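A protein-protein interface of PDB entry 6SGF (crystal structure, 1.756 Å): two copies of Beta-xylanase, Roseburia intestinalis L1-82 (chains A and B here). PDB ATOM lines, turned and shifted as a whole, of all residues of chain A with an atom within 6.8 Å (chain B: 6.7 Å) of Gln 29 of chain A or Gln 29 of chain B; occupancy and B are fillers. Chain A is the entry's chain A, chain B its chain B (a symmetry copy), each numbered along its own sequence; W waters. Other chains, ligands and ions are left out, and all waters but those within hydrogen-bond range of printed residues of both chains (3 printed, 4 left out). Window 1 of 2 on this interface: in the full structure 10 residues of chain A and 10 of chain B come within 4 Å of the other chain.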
ATOM      1  N   ALA A  11      11.356  14.556 -25.805  1.00  0.00           N
ATOM      2  CA  ALA A  11      12.643  13.959 -26.138  1.00  0.00           C
ATOM      3  C   ALA A  11      12.554  12.443 -26.238  1.00  0.00           C
ATOM      4  O   ALA A  11      13.079  11.837 -27.178  1.00  0.00           O
ATOM      5  CB  ALA A  11      13.691  14.342 -25.087  1.00  0.00           C
ATOM      6  N   ASP A  12      11.888  11.808 -25.278  1.00  0.00           N
ATOM      7  CA  ASP A  12      11.843  10.352 -25.271  1.00  0.00           C
ATOM      8  C   ASP A  12      11.035   9.756 -26.417  1.00  0.00           C
ATOM      9  O   ASP A  12      11.065   8.537 -26.591  1.00  0.00           O
ATOM     10  CB  ASP A  12      11.308   9.838 -23.938  1.00  0.00           C
ATOM     11  CG  ASP A  12       9.794   9.858 -23.845  1.00  0.00           C
ATOM     12  OD1 ASP A  12       9.155  10.784 -24.378  1.00  0.00           O
ATOM     13  OD2 ASP A  12       9.246   8.941 -23.186  1.00  0.00           O
ATOM     14  N   GLU A  24      22.885  11.329 -25.006  1.00  0.00           N
ATOM     15  CA  GLU A  24      22.301  10.326 -24.139  1.00  0.00           C
ATOM     16  C   GLU A  24      20.943  10.829 -23.685  1.00  0.00           C
ATOM     17  O   GLU A  24      20.770  12.030 -23.485  1.00  0.00           O
ATOM     18  CB  GLU A  24      23.200  10.048 -22.928  1.00  0.00           C
ATOM     19  CG  GLU A  24      23.514  11.307 -22.119  1.00  0.00           C
ATOM     20  CD  GLU A  24      24.319  11.010 -20.864  1.00  0.00           C
ATOM     21  OE1 GLU A  24      25.545  10.783 -20.955  1.00  0.00           O
ATOM     22  OE2 GLU A  24      23.714  10.982 -19.785  1.00  0.00           O
ATOM     23  N   LEU A  25      19.981   9.929 -23.549  1.00  0.00           N
ATOM     24  CA  LEU A  25      18.663  10.287 -23.035  1.00  0.00           C
ATOM     25  C   LEU A  25      18.715  10.116 -21.526  1.00  0.00           C
ATOM     26  O   LEU A  25      18.837   8.987 -21.027  1.00  0.00           O
ATOM     27  CB  LEU A  25      17.574   9.421 -23.652  1.00  0.00           C
ATOM     28  CG  LEU A  25      16.124   9.717 -23.233  1.00  0.00           C
ATOM     29  CD1 LEU A  25      15.679  11.071 -23.839  1.00  0.00           C
ATOM     30  CD2 LEU A  25      15.240   8.577 -23.670  1.00  0.00           C
ATOM     31  N   ALA A  26      18.657  11.226 -20.808  1.00  0.00           N
ATOM     32  CA  ALA A  26      18.775  11.232 -19.360  1.00  0.00           C
ATOM     33  C   ALA A  26      17.779  12.223 -18.771  1.00  0.00           C
ATOM     34  O   ALA A  26      17.576  13.311 -19.307  1.00  0.00           O
ATOM     35  CB  ALA A  26      20.194  11.580 -18.921  1.00  0.00           C
ATOM     36  N   ASP A  27      17.119  11.819 -17.688  1.00  0.00           N
ATOM     37  CA  ASP A  27      16.144  12.664 -17.004  1.00  0.00           C
ATOM     38  C   ASP A  27      15.128  13.243 -18.003  1.00  0.00           C
ATOM     39  O   ASP A  27      14.687  14.383 -17.901  1.00  0.00           O
ATOM     40  CB  ASP A  27      16.882  13.724 -16.158  1.00  0.00           C
ATOM     41  CG  ASP A  27      17.757  13.062 -15.040  1.00  0.00           C
ATOM     42  OD1 ASP A  27      17.517  11.869 -14.720  1.00  0.00           O
ATOM     43  OD2 ASP A  27      18.689  13.693 -14.469  1.00  0.00           O
ATOM     44  N   GLY A  28      14.749  12.420 -18.979  1.00  0.00           N
ATOM     45  CA  GLY A  28      13.728  12.749 -19.962  1.00  0.00           C
ATOM     46  C   GLY A  28      14.135  13.725 -21.052  1.00  0.00           C
ATOM     47  O   GLY A  28      13.280  14.139 -21.837  1.00  0.00           O
ATOM     48  N   GLN A  29      15.413  14.067 -21.143  1.00  0.00           N
ATOM     49  CA  GLN A  29      15.943  14.997 -22.125  1.00  0.00           C
ATOM     50  C   GLN A  29      17.066  14.331 -22.900  1.00  0.00           C
ATOM     51  O   GLN A  29      17.740  13.435 -22.389  1.00  0.00           O
ATOM     52  CB  GLN A  29      16.481  16.239 -21.460  1.00  0.00           C
ATOM     53  CG  GLN A  29      15.491  16.874 -20.529  1.00  0.00           C
ATOM     54  CD  GLN A  29      15.958  18.152 -19.890  1.00  0.00           C
ATOM     55  OE1 GLN A  29      17.152  18.410 -19.725  1.00  0.00           O
ATOM     56  NE2 GLN A  29      15.007  18.962 -19.501  1.00  0.00           N
ATOM     57  N   TRP A  30      17.237  14.756 -24.149  1.00  0.00           N
ATOM     58  CA  TRP A  30      18.396  14.358 -24.946  1.00  0.00           C
ATOM     59  C   TRP A  30      19.530  15.314 -24.568  1.00  0.00           C
ATOM     60  O   TRP A  30      19.484  16.493 -24.899  1.00  0.00           O
ATOM     61  CB  TRP A  30      18.088  14.404 -26.452  1.00  0.00           C
ATOM     62  CG  TRP A  30      17.443  13.161 -26.974  1.00  0.00           C
ATOM     63  CD1 TRP A  30      16.160  13.031 -27.429  1.00  0.00           C
ATOM     64  CD2 TRP A  30      18.035  11.870 -27.076  1.00  0.00           C
ATOM     65  NE1 TRP A  30      15.927  11.746 -27.809  1.00  0.00           N
ATOM     66  CE2 TRP A  30      17.056  11.003 -27.587  1.00  0.00           C
ATOM     67  CE3 TRP A  30      19.301  11.360 -26.777  1.00  0.00           C
ATOM     68  CZ2 TRP A  30      17.305   9.652 -27.823  1.00  0.00           C
ATOM     69  CZ3 TRP A  30      19.543  10.011 -27.009  1.00  0.00           C
ATOM     70  CH2 TRP A  30      18.555   9.182 -27.521  1.00  0.00           C
ATOM     71  N   LYS A  31      20.531  14.813 -23.855  1.00  0.00           N
ATOM     72  CA  LYS A  31      21.657  15.616 -23.393  1.00  0.00           C
ATOM     73  C   LYS A  31      22.797  15.456 -24.402  1.00  0.00           C
ATOM     74  O   LYS A  31      23.217  14.334 -24.708  1.00  0.00           O
ATOM     75  CB  LYS A  31      22.054  15.198 -21.977  1.00  0.00           C
ATOM     76  CG  LYS A  31      20.943  15.561 -20.944  1.00  0.00           C
ATOM     77  CD  LYS A  31      21.355  15.420 -19.506  1.00  0.00           C
ATOM     78  CE  LYS A  31      20.159  15.631 -18.565  1.00  0.00           C
ATOM     79  NZ  LYS A  31      19.641  17.011 -18.611  1.00  0.00           N
ATOM     80  N   GLN A  60      12.349  23.224 -28.060  1.00  0.00           N
ATOM     81  CA  GLN A  60      12.540  23.627 -26.667  1.00  0.00           C
ATOM     82  C   GLN A  60      13.810  22.994 -26.126  1.00  0.00           C
ATOM     83  O   GLN A  60      13.985  21.774 -26.218  1.00  0.00           O
ATOM     84  CB  GLN A  60      11.336  23.266 -25.797  1.00  0.00           C
ATOM     85  CG  GLN A  60      11.490  23.741 -24.339  1.00  0.00           C
ATOM     86  CD  GLN A  60      10.241  23.461 -23.510  1.00  0.00           C
ATOM     87  OE1 GLN A  60       9.299  22.837 -23.980  1.00  0.00           O
ATOM     88  NE2 GLN A  60      10.249  23.887 -22.282  1.00  0.00           N
ATOM     89  N   VAL A  61      14.689  23.821 -25.557  1.00  0.00           N
ATOM     90  CA  VAL A  61      15.982  23.363 -25.065  1.00  0.00           C
ATOM     91  C   VAL A  61      16.135  23.763 -23.604  1.00  0.00           C
ATOM     92  O   VAL A  61      15.376  24.577 -23.070  1.00  0.00           O
ATOM     93  CB  VAL A  61      17.169  23.898 -25.903  1.00  0.00           C
ATOM     94  CG1 VAL A  61      17.043  23.423 -27.320  1.00  0.00           C
ATOM     95  CG2 VAL A  61      17.302  25.433 -25.847  1.00  0.00           C
ATOM     96  N   ALA A  62      17.123  23.148 -22.954  1.00  0.00           N
ATOM     97  CA  ALA A  62      17.491  23.475 -21.583  1.00  0.00           C
ATOM     98  C   ALA A  62      18.997  23.353 -21.442  1.00  0.00           C
ATOM     99  O   ALA A  62      19.669  22.642 -22.211  1.00  0.00           O
ATOM    100  CB  ALA A  62      16.770  22.561 -20.571  1.00  0.00           C
ATOM    101  N   ASP A  63      19.523  24.092 -20.456  1.00  0.00           N
ATOM    102  CA  ASP A  63      20.942  24.063 -20.098  1.00  0.00           C
ATOM    103  C   ASP A  63      21.828  24.359 -21.309  1.00  0.00           C
ATOM    104  O   ASP A  63      22.850  23.701 -21.548  1.00  0.00           O
ATOM    105  CB  ASP A  63      21.313  22.728 -19.461  1.00  0.00           C
ATOM    106  CG  ASP A  63      21.012  22.714 -17.989  1.00  0.00           C
ATOM    107  OD1 ASP A  63      21.201  23.766 -17.379  1.00  0.00           O
ATOM    108  OD2 ASP A  63      20.546  21.697 -17.475  1.00  0.00           O
ATOM    109  N   SER A 122      20.665  20.577 -23.886  1.00  0.00           N
ATOM    110  CA  SER A 122      19.657  19.529 -23.762  1.00  0.00           C
ATOM    111  C   SER A 122      18.451  19.857 -24.623  1.00  0.00           C
ATOM    112  O   SER A 122      17.965  20.986 -24.616  1.00  0.00           O
ATOM    113  CB  SER A 122      19.173  19.351 -22.308  1.00  0.00           C
ATOM    114  OG  SER A 122      20.252  19.064 -21.446  1.00  0.00           O
ATOM    115  N   LEU A 123      17.941  18.853 -25.331  1.00  0.00           N
ATOM    116  CA  LEU A 123      16.682  18.986 -26.044  1.00  0.00           C
ATOM    117  C   LEU A 123      15.535  18.454 -25.188  1.00  0.00           C
ATOM    118  O   LEU A 123      15.540  17.280 -24.773  1.00  0.00           O
ATOM    119  CB  LEU A 123      16.715  18.246 -27.375  1.00  0.00           C
ATOM    120  CG  LEU A 123      15.429  18.312 -28.199  1.00  0.00           C
ATOM    121  CD1 LEU A 123      15.161  19.675 -28.796  1.00  0.00           C
ATOM    122  CD2 LEU A 123      15.525  17.285 -29.330  1.00  0.00           C
ATOM    123  N   VAL A 124      14.526  19.298 -25.005  1.00  0.00           N
ATOM    124  CA  VAL A 124      13.329  18.996 -24.215  1.00  0.00           C
ATOM    125  C   VAL A 124      12.204  18.451 -25.086  1.00  0.00           C
ATOM    126  O   VAL A 124      11.634  17.398 -24.794  1.00  0.00           O
ATOM    127  CB  VAL A 124      12.860  20.263 -23.462  1.00  0.00           C
ATOM    128  CG1 VAL A 124      11.525  20.026 -22.746  1.00  0.00           C
ATOM    129  CG2 VAL A 124      13.922  20.776 -22.480  1.00  0.00           C
ATOM    130  N   ALA B  11       6.245  21.077 -19.060  1.00  0.00           N
ATOM    131  CA  ALA B  11       6.212  21.738 -17.759  1.00  0.00           C
ATOM    132  C   ALA B  11       6.080  23.253 -17.880  1.00  0.00           C
ATOM    133  O   ALA B  11       5.303  23.874 -17.145  1.00  0.00           O
ATOM    134  CB  ALA B  11       7.453  21.382 -16.942  1.00  0.00           C
ATOM    135  N   ASP B  12       6.806  23.870 -18.814  1.00  0.00           N
ATOM    136  CA  ASP B  12       6.733  25.326 -18.881  1.00  0.00           C
ATOM    137  C   ASP B  12       5.374  25.843 -19.328  1.00  0.00           C
ATOM    138  O   ASP B  12       5.129  27.050 -19.214  1.00  0.00           O
ATOM    139  CB  ASP B  12       7.833  25.894 -19.791  1.00  0.00           C
ATOM    140  CG  ASP B  12       7.577  25.689 -21.265  1.00  0.00           C
ATOM    141  OD1 ASP B  12       7.001  24.655 -21.660  1.00  0.00           O
ATOM    142  OD2 ASP B  12       8.033  26.551 -22.050  1.00  0.00           O
ATOM    143  N   GLU B  24       9.860  24.655  -8.275  1.00  0.00           N
ATOM    144  CA  GLU B  24      10.525  25.647  -9.098  1.00  0.00           C
ATOM    145  C   GLU B  24      10.641  25.062 -10.485  1.00  0.00           C
ATOM    146  O   GLU B  24      10.842  23.850 -10.633  1.00  0.00           O
ATOM    147  CB  GLU B  24      11.920  26.004  -8.546  1.00  0.00           C
ATOM    148  CG  GLU B  24      12.860  24.832  -8.487  1.00  0.00           C
ATOM    149  CD  GLU B  24      13.943  24.997  -7.431  1.00  0.00           C
ATOM    150  OE1 GLU B  24      15.134  24.900  -7.796  1.00  0.00           O
ATOM    151  OE2 GLU B  24      13.602  25.243  -6.246  1.00  0.00           O
ATOM    152  N   LEU B  25      10.478  25.921 -11.481  1.00  0.00           N
ATOM    153  CA  LEU B  25      10.635  25.562 -12.887  1.00  0.00           C
ATOM    154  C   LEU B  25      12.092  25.784 -13.248  1.00  0.00           C
ATOM    155  O   LEU B  25      12.560  26.930 -13.282  1.00  0.00           O
ATOM    156  CB  LEU B  25       9.722  26.412 -13.765  1.00  0.00           C
ATOM    157  CG  LEU B  25       9.743  26.127 -15.256  1.00  0.00           C
ATOM    158  CD1 LEU B  25       9.132  24.746 -15.512  1.00  0.00           C
ATOM    159  CD2 LEU B  25       8.974  27.191 -16.066  1.00  0.00           C
ATOM    160  N   ALA B  26      12.817  24.703 -13.499  1.00  0.00           N
ATOM    161  CA  ALA B  26      14.247  24.797 -13.771  1.00  0.00           C
ATOM    162  C   ALA B  26      14.587  23.796 -14.866  1.00  0.00           C
ATOM    163  O   ALA B  26      14.077  22.673 -14.872  1.00  0.00           O
ATOM    164  CB  ALA B  26      15.100  24.523 -12.518  1.00  0.00           C
ATOM    165  N   ASP B  27      15.411  24.225 -15.818  1.00  0.00           N
ATOM    166  CA  ASP B  27      15.853  23.347 -16.903  1.00  0.00           C
ATOM    167  C   ASP B  27      14.654  22.688 -17.583  1.00  0.00           C
ATOM    168  O   ASP B  27      14.693  21.525 -17.973  1.00  0.00           O
ATOM    169  CB  ASP B  27      16.857  22.313 -16.374  1.00  0.00           C
ATOM    170  CG  ASP B  27      18.149  22.967 -15.897  1.00  0.00           C
ATOM    171  OD1 ASP B  27      18.356  24.129 -16.248  1.00  0.00           O
ATOM    172  OD2 ASP B  27      18.948  22.355 -15.180  1.00  0.00           O
ATOM    173  N   GLY B  28      13.578  23.454 -17.723  1.00  0.00           N
ATOM    174  CA  GLY B  28      12.396  23.025 -18.425  1.00  0.00           C
ATOM    175  C   GLY B  28      11.517  22.025 -17.688  1.00  0.00           C
ATOM    176  O   GLY B  28      10.562  21.526 -18.273  1.00  0.00           O
ATOM    177  N   GLN B  29      11.794  21.744 -16.419  1.00  0.00           N
ATOM    178  CA  GLN B  29      10.999  20.808 -15.629  1.00  0.00           C
ATOM    179  C   GLN B  29      10.510  21.459 -14.341  1.00  0.00           C
ATOM    180  O   GLN B  29      11.149  22.351 -13.788  1.00  0.00           O
ATOM    181  CB  GLN B  29      11.832  19.568 -15.280  1.00  0.00           C
ATOM    182  CG  GLN B  29      12.314  18.859 -16.535  1.00  0.00           C
ATOM    183  CD  GLN B  29      13.148  17.623 -16.239  1.00  0.00           C
ATOM    184  OE1 GLN B  29      13.571  17.401 -15.095  1.00  0.00           O
ATOM    185  NE2 GLN B  29      13.421  16.840 -17.279  1.00  0.00           N
ATOM    186  N   TRP B  30       9.357  21.010 -13.863  1.00  0.00           N
ATOM    187  CA  TRP B  30       8.893  21.430 -12.548  1.00  0.00           C
ATOM    188  C   TRP B  30       9.582  20.529 -11.526  1.00  0.00           C
ATOM    189  O   TRP B  30       9.284  19.333 -11.459  1.00  0.00           O
ATOM    190  CB  TRP B  30       7.371  21.327 -12.452  1.00  0.00           C
ATOM    191  CG  TRP B  30       6.621  22.534 -12.932  1.00  0.00           C
ATOM    192  CD1 TRP B  30       5.804  22.615 -14.023  1.00  0.00           C
ATOM    193  CD2 TRP B  30       6.635  23.838 -12.343  1.00  0.00           C
ATOM    194  NE1 TRP B  30       5.288  23.887 -14.140  1.00  0.00           N
ATOM    195  CE2 TRP B  30       5.794  24.660 -13.126  1.00  0.00           C
ATOM    196  CE3 TRP B  30       7.286  24.396 -11.228  1.00  0.00           C
ATOM    197  CZ2 TRP B  30       5.580  26.011 -12.831  1.00  0.00           C
ATOM    198  CZ3 TRP B  30       7.070  25.744 -10.937  1.00  0.00           C
ATOM    199  CH2 TRP B  30       6.213  26.527 -11.727  1.00  0.00           C
ATOM    200  N   LYS B  31      10.508  21.099 -10.735  1.00  0.00           N
ATOM    201  CA  LYS B  31      11.282  20.360  -9.745  1.00  0.00           C
ATOM    202  C   LYS B  31      10.591  20.508  -8.391  1.00  0.00           C
ATOM    203  O   LYS B  31      10.364  21.625  -7.920  1.00  0.00           O
ATOM    204  CB  LYS B  31      12.735  20.846  -9.694  1.00  0.00           C
ATOM    205  CG  LYS B  31      13.460  20.704 -11.055  1.00  0.00           C
ATOM    206  CD  LYS B  31      14.944  20.504 -10.978  1.00  0.00           C
ATOM    207  CE  LYS B  31      15.513  20.282 -12.384  1.00  0.00           C
ATOM    208  NZ  LYS B  31      15.469  18.884 -12.797  1.00  0.00           N
ATOM    209  N   GLN B  60       4.601  12.318 -17.359  1.00  0.00           N
ATOM    210  CA  GLN B  60       6.007  11.978 -17.511  1.00  0.00           C
ATOM    211  C   GLN B  60       6.817  12.674 -16.427  1.00  0.00           C
ATOM    212  O   GLN B  60       6.719  13.902 -16.260  1.00  0.00           O
ATOM    213  CB  GLN B  60       6.520  12.376 -18.894  1.00  0.00           C
ATOM    214  CG  GLN B  60       7.976  11.978 -19.155  1.00  0.00           C
ATOM    215  CD  GLN B  60       8.442  12.295 -20.589  1.00  0.00           C
ATOM    216  OE1 GLN B  60       7.783  13.013 -21.344  1.00  0.00           O
ATOM    217  NE2 GLN B  60       9.575  11.762 -20.946  1.00  0.00           N
ATOM    218  N   VAL B  61       7.616  11.888 -15.704  1.00  0.00           N
ATOM    219  CA  VAL B  61       8.434  12.370 -14.603  1.00  0.00           C
ATOM    220  C   VAL B  61       9.897  11.980 -14.811  1.00  0.00           C
ATOM    221  O   VAL B  61      10.239  11.121 -15.632  1.00  0.00           O
ATOM    222  CB  VAL B  61       7.928  11.864 -13.240  1.00  0.00           C
ATOM    223  CG1 VAL B  61       6.503  12.318 -12.994  1.00  0.00           C
ATOM    224  CG2 VAL B  61       8.042  10.381 -13.147  1.00  0.00           C
ATOM    225  N   ALA B  62      10.763  12.627 -14.032  1.00  0.00           N
ATOM    226  CA  ALA B  62      12.195  12.347 -14.062  1.00  0.00           C
ATOM    227  C   ALA B  62      12.744  12.526 -12.652  1.00  0.00           C
ATOM    228  O   ALA B  62      12.173  13.238 -11.838  1.00  0.00           O
ATOM    229  CB  ALA B  62      12.914  13.253 -15.078  1.00  0.00           C
ATOM    230  N   ASP B  63      13.853  11.848 -12.374  1.00  0.00           N
ATOM    231  CA  ASP B  63      14.544  11.945 -11.084  1.00  0.00           C
ATOM    232  C   ASP B  63      13.599  11.686  -9.909  1.00  0.00           C
ATOM    233  O   ASP B  63      13.650  12.356  -8.873  1.00  0.00           O
ATOM    234  CB  ASP B  63      15.240  13.289 -10.943  1.00  0.00           C
ATOM    235  CG  ASP B  63      16.547  13.323 -11.695  1.00  0.00           C
ATOM    236  OD1 ASP B  63      17.218  12.272 -11.739  1.00  0.00           O
ATOM    237  OD2 ASP B  63      16.854  14.389 -12.228  1.00  0.00           O
ATOM    238  N   SER B 122      10.695  15.347 -10.493  1.00  0.00           N
ATOM    239  CA  SER B 122      10.503  16.373 -11.514  1.00  0.00           C
ATOM    240  C   SER B 122       9.370  15.997 -12.451  1.00  0.00           C
ATOM    241  O   SER B 122       9.278  14.845 -12.890  1.00  0.00           O
ATOM    242  CB  SER B 122      11.775  16.564 -12.326  1.00  0.00           C
ATOM    243  OG  SER B 122      12.816  16.954 -11.478  1.00  0.00           O
ATOM    244  N   LEU B 123       8.520  16.970 -12.783  1.00  0.00           N
ATOM    245  CA  LEU B 123       7.477  16.767 -13.778  1.00  0.00           C
ATOM    246  C   LEU B 123       7.985  17.274 -15.115  1.00  0.00           C
ATOM    247  O   LEU B 123       8.368  18.441 -15.223  1.00  0.00           O
ATOM    248  CB  LEU B 123       6.176  17.478 -13.393  1.00  0.00           C
ATOM    249  CG  LEU B 123       5.081  17.419 -14.463  1.00  0.00           C
ATOM    250  CD1 LEU B 123       4.506  16.040 -14.656  1.00  0.00           C
ATOM    251  CD2 LEU B 123       3.966  18.395 -14.188  1.00  0.00           C
ATOM    252  N   VAL B 124       7.935  16.411 -16.131  1.00  0.00           N
ATOM    253  CA  VAL B 124       8.377  16.706 -17.492  1.00  0.00           C
ATOM    254  C   VAL B 124       7.228  17.158 -18.367  1.00  0.00           C
ATOM    255  O   VAL B 124       7.324  18.164 -19.077  1.00  0.00           O
ATOM    256  CB  VAL B 124       9.060  15.450 -18.093  1.00  0.00           C
ATOM    257  CG1 VAL B 124       9.435  15.668 -19.563  1.00  0.00           C
ATOM    258  CG2 VAL B 124      10.235  15.021 -17.215  1.00  0.00           C
HETATM  259  O   HOH W   1      14.014  24.845 -20.850  1.00  0.00           O
HETATM  260  O   HOH W   2      12.172  10.942 -17.559  1.00  0.00           O
HETATM  261  O   HOH W   3      12.310  17.898 -19.723  1.00  0.00           O
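The side-chain amino group (NZ) of Lys 31 of chain A sits at hydrogen-bond distance from the side-chain amide oxygen (OE1) of Gln 29 of chain A (3.1 Å). The backbone NH (N) of Val 124 of chain A is in hydrogen-bond range of the backbone carbonyl oxygen (O) of Gln 60 of chain A. N of Ser 122 of chain A lies within hydrogen-bond range of O of Ala 62 of chain A (2.8 Å). NZ of Lys 31 of chain B lies within hydrogen-bond range of OE1 of Gln 29 of chain B (3.3 Å). O of Gln 60 of chain B sits at hydrogen-bond distance from N of Val 124 of chain B (2.8 Å). The backbone NH of Ala 62 of chain B is in hydrogen-bond range of the backbone carbonyl oxygen of Ser 122 of chain B (2.9 Å).
Asp 12 of chain A touches Gln 60 of chain B, and with the chains exchanged Gln 60 of chain A touches Asp 12 of chain B. Asp 27 of chain A touches Ala 62 of chain B, and with the chains exchanged Ala 62 of chain A touches Asp 27 of chain B. Asp 27 of chain A touches Asp 63 of chain B, and with the chains exchanged Asp 63 of chain A touches Asp 27 of chain B. Gln 29 of chain A touches its own counterpart, Gln 29 of chain B.
Gln 29 of chain A touches two residues of chain B. Gln 29 of chain B touches just these residues of chain A: Asp 27 and Gln 29. Printed residues of chain B within 4 Å of Asp 63 of chain A: Asp 27. Of the printed residues of chain A, Asp 12 of chain B touches Gln 60. Printed residues of chain B within 4 Å of Ala 62 of chain A: Asp 27 (3.5 Å). Of the printed residues of chain A, Asp 63 of chain B touches Asp 27. Printed residues of chain A within 4 Å of Ala 62 of chain B: Asp 27 (3.5 Å). Val 124 of chain B touches none of the printed residues of chain A. The nearest residue of chain B that does not touch Gln 29 of chain A is Gly 28 of chain B (4.9 Å).
Printed residues of chain B that touch a printed residue of chain A: Asp 12, Asp 27, Gln 29, Gln 60, Ala 62 and Asp 63. Of the 17 printed residues of chain A, 6 touch a printed residue of chain B. Among the printed residues, no Asp or Glu carboxylate lies within 4 Å of a Lys or Arg side-chain nitrogen of the other chain.
The backbone carbonyl oxygen (O) of Asp 27 of chain A sits at hydrogen-bond distance from the side-chain amide nitrogen (NE2) of Gln 29 of chain B (2.8 Å). NE2 of Gln 29 of chain A lies within hydrogen-bond range of O of Asp 27 of chain B (3.0 Å). NE2 of Gln 29 of chain A sits close to NE2 of Gln 29 of chain B. The side-chain carboxylate (OD1) of Asp 12 of chain B sits close to the side-chain amide nitrogen (NE2) of Gln 60 of chain A, at 3.4 Å. The side-chain carboxylate (OD2) of Asp 63 of chain B lies close to the side-chain carboxylate (OD2) of Asp 27 of chain A, 3.0 Å away. OD2 of Asp 63 of chain A sits close to OD2 of Asp 27 of chain B (2.9 Å).
Among the printed residues, merely in contact across the chains: Asp 12 of chain A with Gln 60 of chain B (3.5 Å), Asp 27 of chain A with Ala 62 of chain B (3.5 Å) and Ala 62 of chain A with Asp 27 of chain B (3.5 Å).
Water W1 lies within hydrogen-bond range of the backbone carbonyl oxygen of Val 61 of chain A (2.6 Å) and the backbone NH of Gly 28 of chain B (3.5 Å). Water W2 lies within hydrogen-bond range of the backbone carbonyl oxygen of Val 61 of chain B (2.7 Å) and the backbone NH of Gly 28 of chain A (3.3 Å). Water W3 bridges NE2 of Gln 29 of chain B (2.9 Å) and NE2 of Gln 29 of chain A (2.9 Å).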
